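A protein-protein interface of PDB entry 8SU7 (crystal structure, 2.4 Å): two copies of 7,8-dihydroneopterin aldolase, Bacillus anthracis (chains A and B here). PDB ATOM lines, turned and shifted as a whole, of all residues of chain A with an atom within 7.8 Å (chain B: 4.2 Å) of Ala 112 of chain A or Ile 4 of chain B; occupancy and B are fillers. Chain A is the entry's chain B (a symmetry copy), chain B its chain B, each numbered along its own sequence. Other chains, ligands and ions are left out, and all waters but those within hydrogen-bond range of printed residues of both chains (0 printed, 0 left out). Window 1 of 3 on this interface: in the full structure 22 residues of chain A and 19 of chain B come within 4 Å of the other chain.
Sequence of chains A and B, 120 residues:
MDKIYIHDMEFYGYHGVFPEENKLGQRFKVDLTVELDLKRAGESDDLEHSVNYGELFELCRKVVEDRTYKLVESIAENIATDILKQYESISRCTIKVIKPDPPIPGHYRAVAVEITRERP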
ATOM      1  N   LYS A  29      34.760   3.539 -28.627  1.00  0.00           N
ATOM      2  CA  LYS A  29      35.285   4.795 -28.115  1.00  0.00           C
ATOM      3  C   LYS A  29      35.126   4.835 -26.601  1.00  0.00           C
ATOM      4  O   LYS A  29      34.177   4.276 -26.046  1.00  0.00           O
ATOM      5  CB  LYS A  29      34.553   5.988 -28.735  1.00  0.00           C
ATOM      6  CG  LYS A  29      34.630   6.038 -30.254  1.00  0.00           C
ATOM      7  CD  LYS A  29      33.942   7.278 -30.806  1.00  0.00           C
ATOM      8  CE  LYS A  29      34.666   7.820 -32.028  1.00  0.00           C
ATOM      9  NZ  LYS A  29      34.051   9.081 -32.527  1.00  0.00           N
ATOM     10  N   ASP A  31      35.545   7.535 -23.161  1.00  0.00           N
ATOM     11  CA  ASP A  31      35.795   8.795 -22.475  1.00  0.00           C
ATOM     12  C   ASP A  31      36.173   8.474 -21.036  1.00  0.00           C
ATOM     13  O   ASP A  31      35.480   7.701 -20.369  1.00  0.00           O
ATOM     14  CB  ASP A  31      34.548   9.681 -22.493  1.00  0.00           C
ATOM     15  CG  ASP A  31      34.200  10.165 -23.883  1.00  0.00           C
ATOM     16  OD1 ASP A  31      35.127  10.437 -24.673  1.00  0.00           O
ATOM     17  OD2 ASP A  31      32.996  10.279 -24.187  1.00  0.00           O
ATOM     18  N   VAL A  72      29.956  -4.384 -23.527  1.00  0.00           N
ATOM     19  CA  VAL A  72      30.737  -3.177 -23.299  1.00  0.00           C
ATOM     20  C   VAL A  72      30.735  -2.813 -21.821  1.00  0.00           C
ATOM     21  O   VAL A  72      31.628  -2.092 -21.358  1.00  0.00           O
ATOM     22  CB  VAL A  72      30.223  -2.016 -24.174  1.00  0.00           C
ATOM     23  CG1 VAL A  72      30.010  -2.486 -25.611  1.00  0.00           C
ATOM     24  CG2 VAL A  72      28.944  -1.436 -23.598  1.00  0.00           C
ATOM     25  N   GLU A  73      29.730  -3.274 -21.072  1.00  0.00           N
ATOM     26  CA  GLU A  73      29.719  -3.056 -19.630  1.00  0.00           C
ATOM     27  C   GLU A  73      30.963  -3.653 -18.984  1.00  0.00           C
ATOM     28  O   GLU A  73      31.508  -3.088 -18.029  1.00  0.00           O
ATOM     29  CB  GLU A  73      28.462  -3.677 -19.022  1.00  0.00           C
ATOM     30  CG  GLU A  73      27.187  -2.890 -19.263  1.00  0.00           C
ATOM     31  CD  GLU A  73      26.376  -3.417 -20.428  1.00  0.00           C
ATOM     32  OE1 GLU A  73      26.957  -4.069 -21.315  1.00  0.00           O
ATOM     33  OE2 GLU A  73      25.151  -3.175 -20.465  1.00  0.00           O
ATOM     34  N   ILE A  95      33.954   6.124 -16.273  1.00  0.00           N
ATOM     35  CA  ILE A  95      34.319   5.545 -17.560  1.00  0.00           C
ATOM     36  C   ILE A  95      33.076   5.487 -18.436  1.00  0.00           C
ATOM     37  O   ILE A  95      32.030   4.986 -18.008  1.00  0.00           O
ATOM     38  CB  ILE A  95      34.926   4.142 -17.382  1.00  0.00           C
ATOM     39  CG1 ILE A  95      36.202   4.207 -16.536  1.00  0.00           C
ATOM     40  CG2 ILE A  95      35.224   3.506 -18.736  1.00  0.00           C
ATOM     41  CD1 ILE A  95      37.104   5.392 -16.832  1.00  0.00           C
ATOM     42  N   LYS A  96      33.199   5.985 -19.664  1.00  0.00           N
ATOM     43  CA  LYS A  96      32.134   5.931 -20.657  1.00  0.00           C
ATOM     44  C   LYS A  96      32.665   5.184 -21.871  1.00  0.00           C
ATOM     45  O   LYS A  96      33.672   5.590 -22.458  1.00  0.00           O
ATOM     46  CB  LYS A  96      31.698   7.340 -21.060  1.00  0.00           C
ATOM     47  CG  LYS A  96      30.554   7.378 -22.065  1.00  0.00           C
ATOM     48  CD  LYS A  96      29.988   8.790 -22.202  1.00  0.00           C
ATOM     49  CE  LYS A  96      28.733   8.812 -23.064  1.00  0.00           C
ATOM     50  NZ  LYS A  96      28.025  10.122 -22.999  1.00  0.00           N
ATOM     51  N   VAL A  97      31.993   4.098 -22.243  1.00  0.00           N
ATOM     52  CA  VAL A  97      32.393   3.263 -23.370  1.00  0.00           C
ATOM     53  C   VAL A  97      31.315   3.385 -24.435  1.00  0.00           C
ATOM     54  O   VAL A  97      30.144   3.075 -24.182  1.00  0.00           O
ATOM     55  CB  VAL A  97      32.597   1.800 -22.947  1.00  0.00           C
ATOM     56  CG1 VAL A  97      33.278   1.016 -24.059  1.00  0.00           C
ATOM     57  CG2 VAL A  97      33.415   1.730 -21.664  1.00  0.00           C
ATOM     58  N   ILE A  98      31.708   3.837 -25.621  1.00  0.00           N
ATOM     59  CA  ILE A  98      30.779   4.164 -26.695  1.00  0.00           C
ATOM     60  C   ILE A  98      30.904   3.115 -27.792  1.00  0.00           C
ATOM     61  O   ILE A  98      32.013   2.803 -28.242  1.00  0.00           O
ATOM     62  CB  ILE A  98      31.047   5.575 -27.247  1.00  0.00           C
ATOM     63  CG1 ILE A  98      30.751   6.633 -26.179  1.00  0.00           C
ATOM     64  CG2 ILE A  98      30.195   5.837 -28.488  1.00  0.00           C
ATOM     65  CD1 ILE A  98      31.986   7.180 -25.494  1.00  0.00           C
ATOM     66  N   LYS A  99      29.758   2.595 -28.237  1.00  0.00           N
ATOM     67  CA  LYS A  99      29.657   1.690 -29.378  1.00  0.00           C
ATOM     68  C   LYS A  99      28.979   2.469 -30.497  1.00  0.00           C
ATOM     69  O   LYS A  99      27.741   2.529 -30.559  1.00  0.00           O
ATOM     70  CB  LYS A  99      28.838   0.454 -29.003  1.00  0.00           C
ATOM     71  CG  LYS A  99      29.320  -0.834 -29.642  1.00  0.00           C
ATOM     72  CD  LYS A  99      28.401  -1.993 -29.263  1.00  0.00           C
ATOM     73  CE  LYS A  99      28.890  -3.314 -29.824  1.00  0.00           C
ATOM     74  NZ  LYS A  99      27.874  -4.397 -29.674  1.00  0.00           N
ATOM     75  N   PRO A 100      29.735   3.104 -31.397  1.00  0.00           N
ATOM     76  CA  PRO A 100      29.095   4.002 -32.374  1.00  0.00           C
ATOM     77  C   PRO A 100      28.411   3.299 -33.534  1.00  0.00           C
ATOM     78  O   PRO A 100      27.583   3.931 -34.203  1.00  0.00           O
ATOM     79  CB  PRO A 100      30.257   4.875 -32.870  1.00  0.00           C
ATOM     80  CG  PRO A 100      31.472   3.986 -32.725  1.00  0.00           C
ATOM     81  CD  PRO A 100      31.206   3.092 -31.525  1.00  0.00           C
ATOM     82  N   PRO A 102      26.778  -0.188 -33.746  1.00  0.00           N
ATOM     83  CA  PRO A 102      26.261  -1.480 -33.329  1.00  0.00           C
ATOM     84  C   PRO A 102      25.338  -2.080 -34.391  1.00  0.00           C
ATOM     85  O   PRO A 102      24.939  -1.369 -35.287  1.00  0.00           O
ATOM     86  CB  PRO A 102      25.473  -1.151 -32.060  1.00  0.00           C
ATOM     87  CG  PRO A 102      24.930   0.214 -32.319  1.00  0.00           C
ATOM     88  CD  PRO A 102      26.039   0.898 -33.085  1.00  0.00           C
ATOM     89  N   ALA A 110      24.953   6.874 -31.422  1.00  0.00           N
ATOM     90  CA  ALA A 110      25.692   5.827 -30.730  1.00  0.00           C
ATOM     91  C   ALA A 110      24.854   5.294 -29.578  1.00  0.00           C
ATOM     92  O   ALA A 110      23.864   5.906 -29.169  1.00  0.00           O
ATOM     93  CB  ALA A 110      27.027   6.358 -30.195  1.00  0.00           C
ATOM     94  N   VAL A 111      25.253   4.125 -29.085  1.00  0.00           N
ATOM     95  CA  VAL A 111      24.819   3.607 -27.795  1.00  0.00           C
ATOM     96  C   VAL A 111      26.055   3.567 -26.909  1.00  0.00           C
ATOM     97  O   VAL A 111      27.175   3.371 -27.395  1.00  0.00           O
ATOM     98  CB  VAL A 111      24.159   2.215 -27.899  1.00  0.00           C
ATOM     99  CG1 VAL A 111      22.971   2.273 -28.852  1.00  0.00           C
ATOM    100  CG2 VAL A 111      25.168   1.177 -28.338  1.00  0.00           C
ATOM    101  N   ALA A 112      25.858   3.745 -25.606  1.00  0.00           N
ATOM    102  CA  ALA A 112      26.997   3.850 -24.709  1.00  0.00           C
ATOM    103  C   ALA A 112      26.620   3.391 -23.311  1.00  0.00           C
ATOM    104  O   ALA A 112      25.453   3.437 -22.914  1.00  0.00           O
ATOM    105  CB  ALA A 112      27.514   5.294 -24.654  1.00  0.00           C
ATOM    106  N   VAL A 113      27.631   2.938 -22.576  1.00  0.00           N
ATOM    107  CA  VAL A 113      27.514   2.607 -21.164  1.00  0.00           C
ATOM    108  C   VAL A 113      28.449   3.530 -20.395  1.00  0.00           C
ATOM    109  O   VAL A 113      29.543   3.851 -20.871  1.00  0.00           O
ATOM    110  CB  VAL A 113      27.852   1.125 -20.898  1.00  0.00           C
ATOM    111  CG1 VAL A 113      29.347   0.929 -20.707  1.00  0.00           C
ATOM    112  CG2 VAL A 113      27.077   0.630 -19.688  1.00  0.00           C
ATOM    113  N   GLU A 114      28.037   3.921 -19.192  1.00  0.00           N
ATOM    114  CA  GLU A 114      28.806   4.871 -18.396  1.00  0.00           C
ATOM    115  C   GLU A 114      28.654   4.510 -16.930  1.00  0.00           C
ATOM    116  O   GLU A 114      27.533   4.450 -16.418  1.00  0.00           O
ATOM    117  CB  GLU A 114      28.309   6.297 -18.644  1.00  0.00           C
ATOM    118  CG  GLU A 114      29.144   7.374 -17.973  1.00  0.00           C
ATOM    119  CD  GLU A 114      28.568   8.762 -18.171  1.00  0.00           C
ATOM    120  OE1 GLU A 114      27.492   9.046 -17.605  1.00  0.00           O
ATOM    121  OE2 GLU A 114      29.190   9.570 -18.895  1.00  0.00           O
ATOM    122  N   ILE A 115      29.780   4.283 -16.254  1.00  0.00           N
ATOM    123  CA  ILE A 115      29.783   3.900 -14.851  1.00  0.00           C
ATOM    124  C   ILE A 115      30.710   4.833 -14.086  1.00  0.00           C
ATOM    125  O   ILE A 115      31.622   5.445 -14.646  1.00  0.00           O
ATOM    126  CB  ILE A 115      30.205   2.424 -14.649  1.00  0.00           C
ATOM    127  CG1 ILE A 115      31.723   2.274 -14.788  1.00  0.00           C
ATOM    128  CG2 ILE A 115      29.488   1.523 -15.650  1.00  0.00           C
ATOM    129  CD1 ILE A 115      32.234   0.866 -14.540  1.00  0.00           C
ATOM    130  N   LYS B   3      24.761   3.960 -15.962  1.00  0.00           N
ATOM    131  CA  LYS B   3      23.768   4.421 -16.917  1.00  0.00           C
ATOM    132  C   LYS B   3      24.055   3.866 -18.304  1.00  0.00           C
ATOM    133  O   LYS B   3      25.203   3.595 -18.664  1.00  0.00           O
ATOM    134  CB  LYS B   3      23.750   5.955 -16.991  1.00  0.00           C
ATOM    135  CG  LYS B   3      23.780   6.650 -15.635  1.00  0.00           C
ATOM    136  CD  LYS B   3      23.244   8.075 -15.726  1.00  0.00           C
ATOM    137  CE  LYS B   3      24.326   9.051 -16.162  1.00  0.00           C
ATOM    138  NZ  LYS B   3      25.016   9.675 -14.996  1.00  0.00           N
ATOM    139  N   ILE B   4      22.983   3.703 -19.076  1.00  0.00           N
ATOM    140  CA  ILE B   4      23.049   3.339 -20.485  1.00  0.00           C
ATOM    141  C   ILE B   4      22.516   4.512 -21.287  1.00  0.00           C
ATOM    142  O   ILE B   4      21.466   5.072 -20.948  1.00  0.00           O
ATOM    143  CB  ILE B   4      22.229   2.073 -20.788  1.00  0.00           C
ATOM    144  CG1 ILE B   4      22.516   0.989 -19.752  1.00  0.00           C
ATOM    145  CG2 ILE B   4      22.548   1.565 -22.193  1.00  0.00           C
ATOM    146  CD1 ILE B   4      21.707  -0.281 -19.953  1.00  0.00           C
ATOM    147  N   TYR B   5      23.231   4.884 -22.344  1.00  0.00           N
ATOM    148  CA  TYR B   5      22.825   5.975 -23.216  1.00  0.00           C
ATOM    149  C   TYR B   5      22.477   5.436 -24.599  1.00  0.00           C
ATOM    150  O   TYR B   5      23.045   4.441 -25.056  1.00  0.00           O
ATOM    151  CB  TYR B   5      23.952   7.007 -23.412  1.00  0.00           C
ATOM    152  CG  TYR B   5      24.375   7.783 -22.186  1.00  0.00           C
ATOM    153  CD1 TYR B   5      23.593   8.811 -21.685  1.00  0.00           C
ATOM    154  CD2 TYR B   5      25.572   7.500 -21.543  1.00  0.00           C
ATOM    155  CE1 TYR B   5      23.987   9.529 -20.568  1.00  0.00           C
ATOM    156  CE2 TYR B   5      25.968   8.206 -20.426  1.00  0.00           C
ATOM    157  CZ  TYR B   5      25.171   9.217 -19.941  1.00  0.00           C
ATOM    158  OH  TYR B   5      25.564   9.925 -18.829  1.00  0.00           O
ATOM    159  N   LEU B  32      18.259   9.193 -24.886  1.00  0.00           N
ATOM    160  CA  LEU B  32      17.769   8.316 -23.833  1.00  0.00           C
ATOM    161  C   LEU B  32      18.880   8.061 -22.826  1.00  0.00           C
ATOM    162  O   LEU B  32      20.021   7.772 -23.201  1.00  0.00           O
ATOM    163  CB  LEU B  32      17.284   6.994 -24.445  1.00  0.00           C
ATOM    164  CG  LEU B  32      16.504   5.999 -23.593  1.00  0.00           C
ATOM    165  CD1 LEU B  32      15.924   4.882 -24.473  1.00  0.00           C
ATOM    166  CD2 LEU B  32      17.400   5.434 -22.609  1.00  0.00           C
ATOM    167  N   THR B  33      18.522   8.153 -21.545  1.00  0.00           N
ATOM    168  CA  THR B  33      19.376   7.727 -20.443  1.00  0.00           C
ATOM    169  C   THR B  33      18.550   6.878 -19.488  1.00  0.00           C
ATOM    170  O   THR B  33      17.500   7.322 -19.017  1.00  0.00           O
ATOM    171  CB  THR B  33      19.903   8.956 -19.705  1.00  0.00           C
ATOM    172  OG1 THR B  33      20.130  10.016 -20.645  1.00  0.00           O
ATOM    173  CG2 THR B  33      21.196   8.632 -18.973  1.00  0.00           C
ATOM    174  N   VAL B  34      19.015   5.665 -19.199  1.00  0.00           N
ATOM    175  CA  VAL B  34      18.401   4.817 -18.182  1.00  0.00           C
ATOM    176  C   VAL B  34      19.420   4.577 -17.081  1.00  0.00           C
ATOM    177  O   VAL B  34      20.608   4.381 -17.358  1.00  0.00           O
ATOM    178  CB  VAL B  34      17.875   3.468 -18.718  1.00  0.00           C
ATOM    179  CG1 VAL B  34      17.136   3.650 -19.960  1.00  0.00           C
ATOM    180  CG2 VAL B  34      19.008   2.477 -18.934  1.00  0.00           C
ATOM    181  N   LEU B  36      20.625   2.171 -13.823  1.00  0.00           N
ATOM    182  CA  LEU B  36      20.554   0.792 -13.353  1.00  0.00           C
ATOM    183  C   LEU B  36      21.947   0.357 -12.919  1.00  0.00           C
ATOM    184  O   LEU B  36      22.943   0.802 -13.497  1.00  0.00           O
ATOM    185  CB  LEU B  36      20.006  -0.125 -14.446  1.00  0.00           C
ATOM    186  CG  LEU B  36      20.915  -0.504 -15.612  1.00  0.00           C
ATOM    187  CD1 LEU B  36      20.169  -1.467 -16.545  1.00  0.00           C
ATOM    188  CD2 LEU B  36      21.372   0.718 -16.369  1.00  0.00           C
ATOM    189  N   LEU B  38      24.977  -1.692 -13.100  1.00  0.00           N
ATOM    190  CA  LEU B  38      25.527  -2.536 -14.153  1.00  0.00           C
ATOM    191  C   LEU B  38      26.802  -3.255 -13.729  1.00  0.00           C
ATOM    192  O   LEU B  38      27.484  -3.838 -14.578  1.00  0.00           O
ATOM    193  CB  LEU B  38      25.779  -1.702 -15.410  1.00  0.00           C
ATOM    194  CG  LEU B  38      24.522  -1.338 -16.203  1.00  0.00           C
ATOM    195  CD1 LEU B  38      24.805  -0.298 -17.270  1.00  0.00           C
ATOM    196  CD2 LEU B  38      23.919  -2.598 -16.828  1.00  0.00           C
ATOM    197  N   VAL B  51      20.617  -4.583 -19.728  1.00  0.00           N
ATOM    198  CA  VAL B  51      19.443  -4.351 -20.561  1.00  0.00           C
ATOM    199  C   VAL B  51      19.892  -4.242 -22.012  1.00  0.00           C
ATOM    200  O   VAL B  51      20.824  -3.492 -22.324  1.00  0.00           O
ATOM    201  CB  VAL B  51      18.692  -3.075 -20.131  1.00  0.00           C
ATOM    202  CG1 VAL B  51      17.658  -2.671 -21.180  1.00  0.00           C
ATOM    203  CG2 VAL B  51      18.031  -3.272 -18.771  1.00  0.00           C
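OE1 of Glu 114 of chain A lies within salt-bridge range of NZ of Lys 3 of chain B (3.7 Å).
N of Tyr 5 of chain B lies within hydrogen-bond range of O of Ala 112 of chain A (2.7 Å).
The side-chain hydroxyl of Tyr 5 of chain B is in hydrogen-bond range of the side-chain carboxylate of Glu 114 of chain A, 2.4 Å away.
O of Val 34 of chain B sits at hydrogen-bond distance from N of Ile 4 of chain B (3.0 Å).
N of Asp 31 of chain A is in hydrogen-bond range of O of Lys 96 of chain A, at 2.8 Å.
N of Val 97 of chain A is in hydrogen-bond range of O of Val 113 of chain A (2.8 Å).
O of Val 111 of chain A is in hydrogen-bond range of N of Lys 99 of chain A (2.8 Å).
Glu 73 of chain A touches Leu 38 of chain B.
Lys 96 of chain A touches Tyr 5 of chain B.
Tyr 5 of chain B touches Val 111 of chain A (O to CA, 3.4 Å).
CA of Ile 4 of chain B touches O of Ala 112 of chain A, at 3.4 Å.
Val 113 of chain A touches Lys 3 of chain B.
Val 113 of chain A touches Leu 38 of chain B.
Ala 112 of chain A touches just these residues of chain B: Ile 4 and Tyr 5.
Ile 4 of chain B touches just one residue of chain A: Ala 112 (3.4 Å).
Of the printed residues of chain A, Lys 3 of chain B touches Val 113 (3.5 Å) and Glu 114 (2.9 Å).
Printed residues of chain A within 4 Å of Leu 38 of chain B: Glu 73 (3.9 Å) and Val 113 (3.4 Å).
Of the printed residues of chain B, Glu 114 of chain A touches Lys 3 (2.9 Å) and Tyr 5 (2.4 Å).
Of the printed residues of chain B, Glu 73 of chain A touches Leu 38.
Asp 31 of chain A touches none of the printed residues of chain B.
Val 51 of chain B touches none of the printed residues of chain A.
The nearest residue of chain A that does not touch Ile 4 of chain B is Glu 73 of chain A (4.5 Å).
The nearest printed residue of chain A that does not touch Lys 3 of chain B is Ala 112 of chain A (4.3 Å).
Of the 9 printed residues of chain B, 4 touch a printed residue of chain A.
Among the printed residues, 9 pairs touch across the chains.
No position is printed for both chains.
Of the 9 pairs that touch across the chains among the printed residues, none has its exchanged pair printed and touching as well.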
